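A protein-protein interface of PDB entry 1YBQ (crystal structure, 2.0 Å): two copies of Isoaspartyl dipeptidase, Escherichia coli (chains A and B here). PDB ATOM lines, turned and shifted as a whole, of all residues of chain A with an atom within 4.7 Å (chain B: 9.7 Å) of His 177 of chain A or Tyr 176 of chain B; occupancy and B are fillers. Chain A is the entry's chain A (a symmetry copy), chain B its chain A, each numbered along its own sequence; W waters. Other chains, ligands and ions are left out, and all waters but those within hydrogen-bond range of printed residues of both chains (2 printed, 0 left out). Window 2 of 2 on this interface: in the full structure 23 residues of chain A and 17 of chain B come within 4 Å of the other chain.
Printed residues of chain A that touch a printed residue of chain B: Ala 172, Pro 173, Asp 174 and His 177. Of the 22 printed residues of chain B, 4 touch a printed residue of chain A. Hydrophobic or aromatic side chains of chain B within 4 Å of the printed part of chain A: Tyr 176, Ala 179 and Ala 183. Among the printed residues, 7 pairs touch across the chains.
O of Leu 215 of chain B is in hydrogen-bond range of SG of Cys 219 of chain B. OD1 of Asp 174 of chain A sits at hydrogen-bond distance from ND1 of His 177 of chain A (2.5 Å).
His 177 of chain A touches just one residue of chain B: Tyr 176. Tyr 176 of chain B touches just these residues of chain A: Ala 172 (3.2 Å), Pro 173 (3.9 Å), Asp 174 (3.9 Å) and His 177 (3.9 Å). Asp 174 of chain A touches just one residue of chain B: Tyr 176. No residue of chain B comes within 4 Å of Ala 179 of chain A. Printed residues of chain B within 4 Å of Pro 173 of chain A: Tyr 176. Printed residues of chain A within 4 Å of Ala 183 of chain B: Ala 172 (3.9 Å). Printed residues of chain B within 4 Å of Ala 172 of chain A: Tyr 176 (3.2 Å), Ala 179 (3.8 Å), Ala 183 (3.9 Å) and Cys 219 (3.3 Å). The nearest residue of chain A that does not touch Tyr 176 of chain B is Pro 140 of chain A (4.2 Å).
Ala 172 of chain A touches Ala 179 of chain B, but with the chains exchanged Ala 179 of chain A does not touch Ala 172 of chain B (21.8 Å). Pro 173 of chain A touches Tyr 176 of chain B, but with the chains exchanged Tyr 176 of chain A does not touch Pro 173 of chain B (15.6 Å). Asp 174 of chain A touches Tyr 176 of chain B, but with the chains exchanged Tyr 176 of chain A does not touch Asp 174 of chain B (10.2 Å). His 177 of chain A touches Tyr 176 of chain B, but with the chains exchanged Tyr 176 of chain A does not touch His 177 of chain B (10.3 Å).
Ala 172 of chain A touches Tyr 176 of chain B (O to CE1, 3.2 Å). Ala 172 of chain A touches Ala 179 of chain B. Ala 183 of chain B touches Ala 172 of chain A (CB to CB, 3.9 Å). Cys 219 of chain B touches Ala 172 of chain A. CE1 of Tyr 176 of chain B touches CA of Pro 173 of chain A (3.9 Å). N of Asp 174 of chain A touches CE1 of Tyr 176 of chain B, 3.9 Å away. OH of Tyr 176 of chain B touches CE1 of His 177 of chain A (3.9 Å).
Water W1 lies within hydrogen-bond range of O of Val 139 of chain A (2.5 Å) and OH of Tyr 176 of chain B (2.8 Å). Water W2 lies within hydrogen-bond range of the backbone carbonyl oxygen of Ala 172 of chain A (2.8 Å) and the backbone carbonyl oxygen of Asn 218 of chain B (3.4 Å).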
ATOM      1  N   VAL A 139      16.347  -0.317 -24.644  1.00  0.00           N
ATOM      2  CA  VAL A 139      15.879  -0.922 -25.891  1.00  0.00           C
ATOM      3  C   VAL A 139      16.205  -2.389 -25.763  1.00  0.00           C
ATOM      4  O   VAL A 139      17.344  -2.755 -25.468  1.00  0.00           O
ATOM      5  CB  VAL A 139      16.576  -0.418 -27.163  1.00  0.00           C
ATOM      6  CG1 VAL A 139      16.163  -1.278 -28.357  1.00  0.00           C
ATOM      7  CG2 VAL A 139      16.188   1.036 -27.425  1.00  0.00           C
ATOM      8  N   PRO A 140      15.212  -3.247 -25.940  1.00  0.00           N
ATOM      9  CA  PRO A 140      13.831  -2.945 -26.282  1.00  0.00           C
ATOM     10  C   PRO A 140      13.073  -2.208 -25.194  1.00  0.00           C
ATOM     11  O   PRO A 140      13.291  -2.385 -23.996  1.00  0.00           O
ATOM     12  CB  PRO A 140      13.154  -4.288 -26.474  1.00  0.00           C
ATOM     13  CG  PRO A 140      14.088  -5.324 -25.900  1.00  0.00           C
ATOM     14  CD  PRO A 140      15.463  -4.700 -25.850  1.00  0.00           C
ATOM     15  N   ALA A 172      22.840  -1.136 -25.640  1.00  0.00           N
ATOM     16  CA  ALA A 172      23.552  -1.739 -26.752  1.00  0.00           C
ATOM     17  C   ALA A 172      22.621  -2.367 -27.813  1.00  0.00           C
ATOM     18  O   ALA A 172      22.810  -3.514 -28.259  1.00  0.00           O
ATOM     19  CB  ALA A 172      24.603  -2.725 -26.240  1.00  0.00           C
ATOM     20  N   PRO A 173      21.586  -1.640 -28.256  1.00  0.00           N
ATOM     21  CA  PRO A 173      20.729  -2.264 -29.240  1.00  0.00           C
ATOM     22  C   PRO A 173      21.465  -2.332 -30.565  1.00  0.00           C
ATOM     23  O   PRO A 173      22.402  -1.561 -30.880  1.00  0.00           O
ATOM     24  CB  PRO A 173      19.531  -1.338 -29.425  1.00  0.00           C
ATOM     25  CG  PRO A 173      20.103   0.036 -29.143  1.00  0.00           C
ATOM     26  CD  PRO A 173      21.357  -0.169 -28.287  1.00  0.00           C
ATOM     27  N   ASP A 174      20.991  -3.292 -31.327  1.00  0.00           N
ATOM     28  CA  ASP A 174      21.459  -3.520 -32.678  1.00  0.00           C
ATOM     29  C   ASP A 174      20.457  -2.860 -33.614  1.00  0.00           C
ATOM     30  O   ASP A 174      19.308  -2.518 -33.261  1.00  0.00           O
ATOM     31  CB  ASP A 174      21.584  -5.029 -33.028  1.00  0.00           C
ATOM     32  CG  ASP A 174      20.314  -5.798 -32.751  1.00  0.00           C
ATOM     33  OD1 ASP A 174      19.336  -5.284 -32.246  1.00  0.00           O
ATOM     34  OD2 ASP A 174      20.362  -7.056 -33.127  1.00  0.00           O
ATOM     35  N   VAL A 175      20.905  -2.720 -34.829  1.00  0.00           N
ATOM     36  CA  VAL A 175      20.093  -2.110 -35.848  1.00  0.00           C
ATOM     37  C   VAL A 175      18.664  -2.658 -35.932  1.00  0.00           C
ATOM     38  O   VAL A 175      17.698  -1.875 -36.034  1.00  0.00           O
ATOM     39  CB  VAL A 175      20.835  -2.176 -37.166  1.00  0.00           C
ATOM     40  CG1 VAL A 175      20.618  -3.550 -37.777  1.00  0.00           C
ATOM     41  CG2 VAL A 175      20.306  -1.094 -38.078  1.00  0.00           C
ATOM     42  N   TYR A 176      18.509  -3.993 -35.881  1.00  0.00           N
ATOM     43  CA  TYR A 176      17.162  -4.561 -35.980  1.00  0.00           C
ATOM     44  C   TYR A 176      16.197  -4.049 -34.890  1.00  0.00           C
ATOM     45  O   TYR A 176      15.012  -3.763 -35.122  1.00  0.00           O
ATOM     46  CB  TYR A 176      17.103  -6.120 -36.068  1.00  0.00           C
ATOM     47  CG  TYR A 176      15.666  -6.643 -35.980  1.00  0.00           C
ATOM     48  CD1 TYR A 176      14.779  -6.475 -37.048  1.00  0.00           C
ATOM     49  CD2 TYR A 176      15.176  -7.242 -34.815  1.00  0.00           C
ATOM     50  CE1 TYR A 176      13.449  -6.893 -36.973  1.00  0.00           C
ATOM     51  CE2 TYR A 176      13.848  -7.661 -34.705  1.00  0.00           C
ATOM     52  CZ  TYR A 176      12.994  -7.489 -35.795  1.00  0.00           C
ATOM     53  OH  TYR A 176      11.710  -7.920 -35.714  1.00  0.00           O
ATOM     54  N   HIS A 177      16.709  -3.989 -33.686  1.00  0.00           N
ATOM     55  CA  HIS A 177      15.905  -3.557 -32.575  1.00  0.00           C
ATOM     56  C   HIS A 177      15.488  -2.141 -32.762  1.00  0.00           C
ATOM     57  O   HIS A 177      14.352  -1.784 -32.506  1.00  0.00           O
ATOM     58  CB  HIS A 177      16.630  -3.732 -31.232  1.00  0.00           C
ATOM     59  CG  HIS A 177      16.402  -5.146 -30.799  1.00  0.00           C
ATOM     60  ND1 HIS A 177      17.284  -6.166 -31.146  1.00  0.00           N
ATOM     61  CD2 HIS A 177      15.356  -5.708 -30.114  1.00  0.00           C
ATOM     62  CE1 HIS A 177      16.776  -7.300 -30.667  1.00  0.00           C
ATOM     63  NE2 HIS A 177      15.619  -7.063 -30.039  1.00  0.00           N
ATOM     64  N   LEU A 178      16.424  -1.347 -33.239  1.00  0.00           N
ATOM     65  CA  LEU A 178      16.122   0.046 -33.427  1.00  0.00           C
ATOM     66  C   LEU A 178      15.074   0.240 -34.486  1.00  0.00           C
ATOM     67  O   LEU A 178      14.095   0.971 -34.286  1.00  0.00           O
ATOM     68  CB  LEU A 178      17.396   0.770 -33.870  1.00  0.00           C
ATOM     69  CG  LEU A 178      18.334   1.030 -32.727  1.00  0.00           C
ATOM     70  CD1 LEU A 178      19.438   1.918 -33.273  1.00  0.00           C
ATOM     71  CD2 LEU A 178      17.599   1.723 -31.579  1.00  0.00           C
ATOM     72  N   ALA A 179      15.336  -0.411 -35.621  1.00  0.00           N
ATOM     73  CA  ALA A 179      14.469  -0.357 -36.782  1.00  0.00           C
ATOM     74  C   ALA A 179      13.039  -0.765 -36.419  1.00  0.00           C
ATOM     75  O   ALA A 179      12.073  -0.070 -36.687  1.00  0.00           O
ATOM     76  CB  ALA A 179      15.043  -1.217 -37.906  1.00  0.00           C
ATOM     77  N   ASN A 180      12.904  -1.916 -35.813  1.00  0.00           N
ATOM     78  CA  ASN A 180      11.591  -2.379 -35.444  1.00  0.00           C
ATOM     79  C   ASN A 180      10.813  -1.395 -34.542  1.00  0.00           C
ATOM     80  O   ASN A 180       9.599  -1.123 -34.682  1.00  0.00           O
ATOM     81  CB  ASN A 180      11.723  -3.767 -34.768  1.00  0.00           C
ATOM     82  CG  ASN A 180      10.386  -4.227 -34.200  1.00  0.00           C
ATOM     83  OD1 ASN A 180       9.372  -4.360 -34.923  1.00  0.00           O
ATOM     84  ND2 ASN A 180      10.370  -4.452 -32.889  1.00  0.00           N
ATOM     85  N   MET A 181      11.542  -0.880 -33.558  1.00  0.00           N
ATOM     86  CA  MET A 181      10.962   0.030 -32.607  1.00  0.00           C
ATOM     87  C   MET A 181      10.429   1.241 -33.310  1.00  0.00           C
ATOM     88  O   MET A 181       9.334   1.697 -33.033  1.00  0.00           O
ATOM     89  CB  MET A 181      12.017   0.448 -31.594  1.00  0.00           C
ATOM     90  CG  MET A 181      11.615   1.615 -30.717  1.00  0.00           C
ATOM     91  SD  MET A 181      12.936   2.110 -29.570  1.00  0.00           S
ATOM     92  CE  MET A 181      14.087   2.749 -30.802  1.00  0.00           C
ATOM     93  N   VAL B 139      24.398 -17.847 -21.337  1.00  0.00           N
ATOM     94  CA  VAL B 139      24.011 -16.567 -21.927  1.00  0.00           C
ATOM     95  C   VAL B 139      22.949 -16.907 -22.943  1.00  0.00           C
ATOM     96  O   VAL B 139      23.152 -17.769 -23.798  1.00  0.00           O
ATOM     97  CB  VAL B 139      25.129 -15.830 -22.678  1.00  0.00           C
ATOM     98  CG1 VAL B 139      24.548 -14.632 -23.430  1.00  0.00           C
ATOM     99  CG2 VAL B 139      26.185 -15.344 -21.688  1.00  0.00           C
ATOM    100  N   PRO B 140      21.791 -16.270 -22.843  1.00  0.00           N
ATOM    101  CA  PRO B 140      21.425 -15.243 -21.881  1.00  0.00           C
ATOM    102  C   PRO B 140      21.337 -15.741 -20.451  1.00  0.00           C
ATOM    103  O   PRO B 140      20.973 -16.881 -20.165  1.00  0.00           O
ATOM    104  CB  PRO B 140      20.039 -14.780 -22.285  1.00  0.00           C
ATOM    105  CG  PRO B 140      19.515 -15.800 -23.265  1.00  0.00           C
ATOM    106  CD  PRO B 140      20.713 -16.538 -23.817  1.00  0.00           C
ATOM    107  N   ALA B 172      27.329 -20.438 -26.678  1.00  0.00           N
ATOM    108  CA  ALA B 172      27.510 -19.890 -28.010  1.00  0.00           C
ATOM    109  C   ALA B 172      26.816 -18.525 -28.215  1.00  0.00           C
ATOM    110  O   ALA B 172      26.102 -18.292 -29.208  1.00  0.00           O
ATOM    111  CB  ALA B 172      27.104 -20.917 -29.068  1.00  0.00           C
ATOM    112  N   PRO B 173      26.999 -17.576 -27.287  1.00  0.00           N
ATOM    113  CA  PRO B 173      26.325 -16.316 -27.506  1.00  0.00           C
ATOM    114  C   PRO B 173      27.013 -15.577 -28.639  1.00  0.00           C
ATOM    115  O   PRO B 173      28.206 -15.769 -28.971  1.00  0.00           O
ATOM    116  CB  PRO B 173      26.517 -15.492 -26.236  1.00  0.00           C
ATOM    117  CG  PRO B 173      27.849 -15.976 -25.702  1.00  0.00           C
ATOM    118  CD  PRO B 173      28.088 -17.369 -26.291  1.00  0.00           C
ATOM    119  N   ASP B 174      26.199 -14.719 -29.214  1.00  0.00           N
ATOM    120  CA  ASP B 174      26.626 -13.825 -30.270  1.00  0.00           C
ATOM    121  C   ASP B 174      26.909 -12.477 -29.623  1.00  0.00           C
ATOM    122  O   ASP B 174      26.502 -12.161 -28.485  1.00  0.00           O
ATOM    123  CB  ASP B 174      25.559 -13.655 -31.386  1.00  0.00           C
ATOM    124  CG  ASP B 174      24.207 -13.256 -30.844  1.00  0.00           C
ATOM    125  OD1 ASP B 174      23.986 -13.152 -29.653  1.00  0.00           O
ATOM    126  OD2 ASP B 174      23.312 -13.012 -31.774  1.00  0.00           O
ATOM    127  N   VAL B 175      27.588 -11.673 -30.391  1.00  0.00           N
ATOM    128  CA  VAL B 175      27.950 -10.355 -29.940  1.00  0.00           C
ATOM    129  C   VAL B 175      26.796  -9.557 -29.322  1.00  0.00           C
ATOM    130  O   VAL B 175      26.967  -8.932 -28.257  1.00  0.00           O
ATOM    131  CB  VAL B 175      28.640  -9.626 -31.073  1.00  0.00           C
ATOM    132  CG1 VAL B 175      27.580  -9.048 -31.996  1.00  0.00           C
ATOM    133  CG2 VAL B 175      29.502  -8.529 -30.494  1.00  0.00           C
ATOM    134  N   TYR B 176      25.617  -9.574 -29.969  1.00  0.00           N
ATOM    135  CA  TYR B 176      24.492  -8.806 -29.425  1.00  0.00           C
ATOM    136  C   TYR B 176      24.114  -9.207 -27.984  1.00  0.00           C
ATOM    137  O   TYR B 176      23.805  -8.377 -27.115  1.00  0.00           O
ATOM    138  CB  TYR B 176      23.219  -8.764 -30.329  1.00  0.00           C
ATOM    139  CG  TYR B 176      22.033  -8.107 -29.614  1.00  0.00           C
ATOM    140  CD1 TYR B 176      22.012  -6.727 -29.391  1.00  0.00           C
ATOM    141  CD2 TYR B 176      20.974  -8.866 -29.107  1.00  0.00           C
ATOM    142  CE1 TYR B 176      20.970  -6.111 -28.695  1.00  0.00           C
ATOM    143  CE2 TYR B 176      19.923  -8.281 -28.397  1.00  0.00           C
ATOM    144  CZ  TYR B 176      19.927  -6.898 -28.203  1.00  0.00           C
ATOM    145  OH  TYR B 176      18.897  -6.312 -27.542  1.00  0.00           O
ATOM    146  N   HIS B 177      24.093 -10.497 -27.758  1.00  0.00           N
ATOM    147  CA  HIS B 177      23.727 -11.003 -26.464  1.00  0.00           C
ATOM    148  C   HIS B 177      24.717 -10.568 -25.442  1.00  0.00           C
ATOM    149  O   HIS B 177      24.355 -10.175 -24.347  1.00  0.00           O
ATOM    150  CB  HIS B 177      23.584 -12.533 -26.458  1.00  0.00           C
ATOM    151  CG  HIS B 177      22.197 -12.839 -26.929  1.00  0.00           C
ATOM    152  ND1 HIS B 177      21.914 -13.048 -28.276  1.00  0.00           N
ATOM    153  CD2 HIS B 177      21.015 -12.896 -26.236  1.00  0.00           C
ATOM    154  CE1 HIS B 177      20.600 -13.235 -28.373  1.00  0.00           C
ATOM    155  NE2 HIS B 177      20.027 -13.154 -27.167  1.00  0.00           N
ATOM    156  N   LEU B 178      25.973 -10.620 -25.833  1.00  0.00           N
ATOM    157  CA  LEU B 178      27.004 -10.245 -24.904  1.00  0.00           C
ATOM    158  C   LEU B 178      26.919  -8.787 -24.551  1.00  0.00           C
ATOM    159  O   LEU B 178      26.957  -8.413 -23.372  1.00  0.00           O
ATOM    160  CB  LEU B 178      28.367 -10.506 -25.550  1.00  0.00           C
ATOM    161  CG  LEU B 178      28.743 -11.959 -25.526  1.00  0.00           C
ATOM    162  CD1 LEU B 178      30.181 -12.038 -26.006  1.00  0.00           C
ATOM    163  CD2 LEU B 178      28.614 -12.522 -24.109  1.00  0.00           C
ATOM    164  N   ALA B 179      26.836  -7.985 -25.615  1.00  0.00           N
ATOM    165  CA  ALA B 179      26.757  -6.541 -25.513  1.00  0.00           C
ATOM    166  C   ALA B 179      25.593  -6.116 -24.614  1.00  0.00           C
ATOM    167  O   ALA B 179      25.738  -5.353 -23.673  1.00  0.00           O
ATOM    168  CB  ALA B 179      26.661  -5.921 -26.905  1.00  0.00           C
ATOM    169  N   ASN B 180      24.420  -6.608 -24.918  1.00  0.00           N
ATOM    170  CA  ASN B 180      23.270  -6.253 -24.127  1.00  0.00           C
ATOM    171  C   ASN B 180      23.424  -6.572 -22.624  1.00  0.00           C
ATOM    172  O   ASN B 180      23.063  -5.805 -21.702  1.00  0.00           O
ATOM    173  CB  ASN B 180      22.022  -6.954 -24.720  1.00  0.00           C
ATOM    174  CG  ASN B 180      20.807  -6.754 -23.822  1.00  0.00           C
ATOM    175  OD1 ASN B 180      20.379  -5.614 -23.533  1.00  0.00           O
ATOM    176  ND2 ASN B 180      20.254  -7.871 -23.355  1.00  0.00           N
ATOM    177  N   MET B 181      23.943  -7.770 -22.381  1.00  0.00           N
ATOM    178  CA  MET B 181      24.124  -8.237 -21.033  1.00  0.00           C
ATOM    179  C   MET B 181      25.031  -7.311 -20.282  1.00  0.00           C
ATOM    180  O   MET B 181      24.766  -6.953 -19.149  1.00  0.00           O
ATOM    181  CB  MET B 181      24.725  -9.635 -21.056  1.00  0.00           C
ATOM    182  CG  MET B 181      25.227 -10.122 -19.713  1.00  0.00           C
ATOM    183  SD  MET B 181      25.988 -11.770 -19.811  1.00  0.00           S
ATOM    184  CE  MET B 181      27.437 -11.300 -20.776  1.00  0.00           C
ATOM    185  N   ALA B 182      26.129  -6.950 -20.934  1.00  0.00           N
ATOM    186  CA  ALA B 182      27.102  -6.054 -20.343  1.00  0.00           C
ATOM    187  C   ALA B 182      26.527  -4.658 -20.040  1.00  0.00           C
ATOM    188  O   ALA B 182      26.772  -4.008 -19.001  1.00  0.00           O
ATOM    189  CB  ALA B 182      28.284  -5.928 -21.314  1.00  0.00           C
ATOM    190  N   ALA B 183      25.773  -4.184 -21.021  1.00  0.00           N
ATOM    191  CA  ALA B 183      25.152  -2.889 -20.956  1.00  0.00           C
ATOM    192  C   ALA B 183      24.155  -2.833 -19.789  1.00  0.00           C
ATOM    193  O   ALA B 183      24.069  -1.857 -19.046  1.00  0.00           O
ATOM    194  CB  ALA B 183      24.503  -2.623 -22.304  1.00  0.00           C
ATOM    195  N   GLU B 184      23.418  -3.943 -19.630  1.00  0.00           N
ATOM    196  CA  GLU B 184      22.430  -4.030 -18.555  1.00  0.00           C
ATOM    197  C   GLU B 184      23.096  -4.020 -17.201  1.00  0.00           C
ATOM    198  O   GLU B 184      22.569  -3.461 -16.247  1.00  0.00           O
ATOM    199  CB  GLU B 184      21.712  -5.369 -18.683  1.00  0.00           C
ATOM    200  CG  GLU B 184      20.667  -5.228 -19.788  1.00  0.00           C
ATOM    201  CD  GLU B 184      19.405  -5.968 -19.457  1.00  0.00           C
ATOM    202  OE1 GLU B 184      19.249  -6.705 -18.510  1.00  0.00           O
ATOM    203  OE2 GLU B 184      18.484  -5.752 -20.325  1.00  0.00           O
ATOM    204  N   PRO B 211      35.867 -12.088 -28.697  1.00  0.00           N
ATOM    205  CA  PRO B 211      34.523 -11.709 -28.312  1.00  0.00           C
ATOM    206  C   PRO B 211      34.508 -10.409 -27.512  1.00  0.00           C
ATOM    207  O   PRO B 211      33.605  -9.595 -27.715  1.00  0.00           O
ATOM    208  CB  PRO B 211      33.953 -12.877 -27.507  1.00  0.00           C
ATOM    209  CG  PRO B 211      34.974 -14.005 -27.583  1.00  0.00           C
ATOM    210  CD  PRO B 211      36.240 -13.432 -28.179  1.00  0.00           C
ATOM    211  N   ASP B 214      35.076  -7.540 -29.974  1.00  0.00           N
ATOM    212  CA  ASP B 214      33.892  -7.378 -30.807  1.00  0.00           C
ATOM    213  C   ASP B 214      32.882  -6.591 -30.013  1.00  0.00           C
ATOM    214  O   ASP B 214      32.333  -5.598 -30.480  1.00  0.00           O
ATOM    215  CB  ASP B 214      33.256  -8.755 -31.188  1.00  0.00           C
ATOM    216  CG  ASP B 214      34.025  -9.617 -32.173  1.00  0.00           C
ATOM    217  OD1 ASP B 214      34.963  -9.201 -32.847  1.00  0.00           O
ATOM    218  OD2 ASP B 214      33.562 -10.853 -32.248  1.00  0.00           O
ATOM    219  N   LEU B 215      32.647  -7.071 -28.784  1.00  0.00           N
ATOM    220  CA  LEU B 215      31.703  -6.443 -27.886  1.00  0.00           C
ATOM    221  C   LEU B 215      32.016  -4.959 -27.757  1.00  0.00           C
ATOM    222  O   LEU B 215      31.163  -4.090 -27.826  1.00  0.00           O
ATOM    223  CB  LEU B 215      31.733  -7.153 -26.527  1.00  0.00           C
ATOM    224  CG  LEU B 215      30.781  -6.572 -25.505  1.00  0.00           C
ATOM    225  CD1 LEU B 215      30.402  -7.686 -24.544  1.00  0.00           C
ATOM    226  CD2 LEU B 215      31.509  -5.475 -24.746  1.00  0.00           C
ATOM    227  N   LEU B 216      33.283  -4.665 -27.586  1.00  0.00           N
ATOM    228  CA  LEU B 216      33.644  -3.274 -27.470  1.00  0.00           C
ATOM    229  C   LEU B 216      33.222  -2.505 -28.695  1.00  0.00           C
ATOM    230  O   LEU B 216      32.635  -1.430 -28.595  1.00  0.00           O
ATOM    231  CB  LEU B 216      35.129  -3.058 -27.160  1.00  0.00           C
ATOM    232  CG  LEU B 216      35.476  -3.513 -25.741  1.00  0.00           C
ATOM    233  CD1 LEU B 216      36.994  -3.574 -25.561  1.00  0.00           C
ATOM    234  CD2 LEU B 216      34.854  -2.578 -24.708  1.00  0.00           C
ATOM    235  N   GLU B 217      33.501  -3.064 -29.864  1.00  0.00           N
ATOM    236  CA  GLU B 217      33.105  -2.341 -31.058  1.00  0.00           C
ATOM    237  C   GLU B 217      31.602  -2.247 -31.250  1.00  0.00           C
ATOM    238  O   GLU B 217      31.159  -1.603 -32.193  1.00  0.00           O
ATOM    239  CB  GLU B 217      33.746  -2.904 -32.326  1.00  0.00           C
ATOM    240  CG  GLU B 217      35.177  -2.383 -32.451  1.00  0.00           C
ATOM    241  CD  GLU B 217      36.074  -3.460 -32.954  1.00  0.00           C
ATOM    242  OE1 GLU B 217      36.037  -3.829 -34.130  1.00  0.00           O
ATOM    243  OE2 GLU B 217      36.846  -3.964 -31.987  1.00  0.00           O
ATOM    244  N   ASN B 218      30.826  -2.881 -30.373  1.00  0.00           N
ATOM    245  CA  ASN B 218      29.382  -2.885 -30.542  1.00  0.00           C
ATOM    246  C   ASN B 218      28.514  -2.287 -29.447  1.00  0.00           C
ATOM    247  O   ASN B 218      27.275  -2.413 -29.431  1.00  0.00           O
ATOM    248  CB  ASN B 218      28.855  -4.268 -30.930  1.00  0.00           C
ATOM    249  CG  ASN B 218      28.889  -4.487 -32.427  1.00  0.00           C
ATOM    250  OD1 ASN B 218      27.852  -4.421 -33.110  1.00  0.00           O
ATOM    251  ND2 ASN B 218      30.095  -4.740 -32.940  1.00  0.00           N
ATOM    252  N   CYS B 219      29.153  -1.621 -28.524  1.00  0.00           N
ATOM    253  CA  CYS B 219      28.386  -0.974 -27.476  1.00  0.00           C
ATOM    254  C   CYS B 219      29.289   0.110 -26.886  1.00  0.00           C
ATOM    255  O   CYS B 219      30.393   0.341 -27.415  1.00  0.00           O
ATOM    256  CB  CYS B 219      27.848  -1.977 -26.450  1.00  0.00           C
ATOM    257  SG  CYS B 219      29.237  -2.704 -25.527  1.00  0.00           S
HETATM  258  O   HOH W   1      19.316  -3.658 -26.746  1.00  0.00           O
HETATM  259  O   HOH W   2      24.616  -4.351 -30.258  1.00  0.00           O
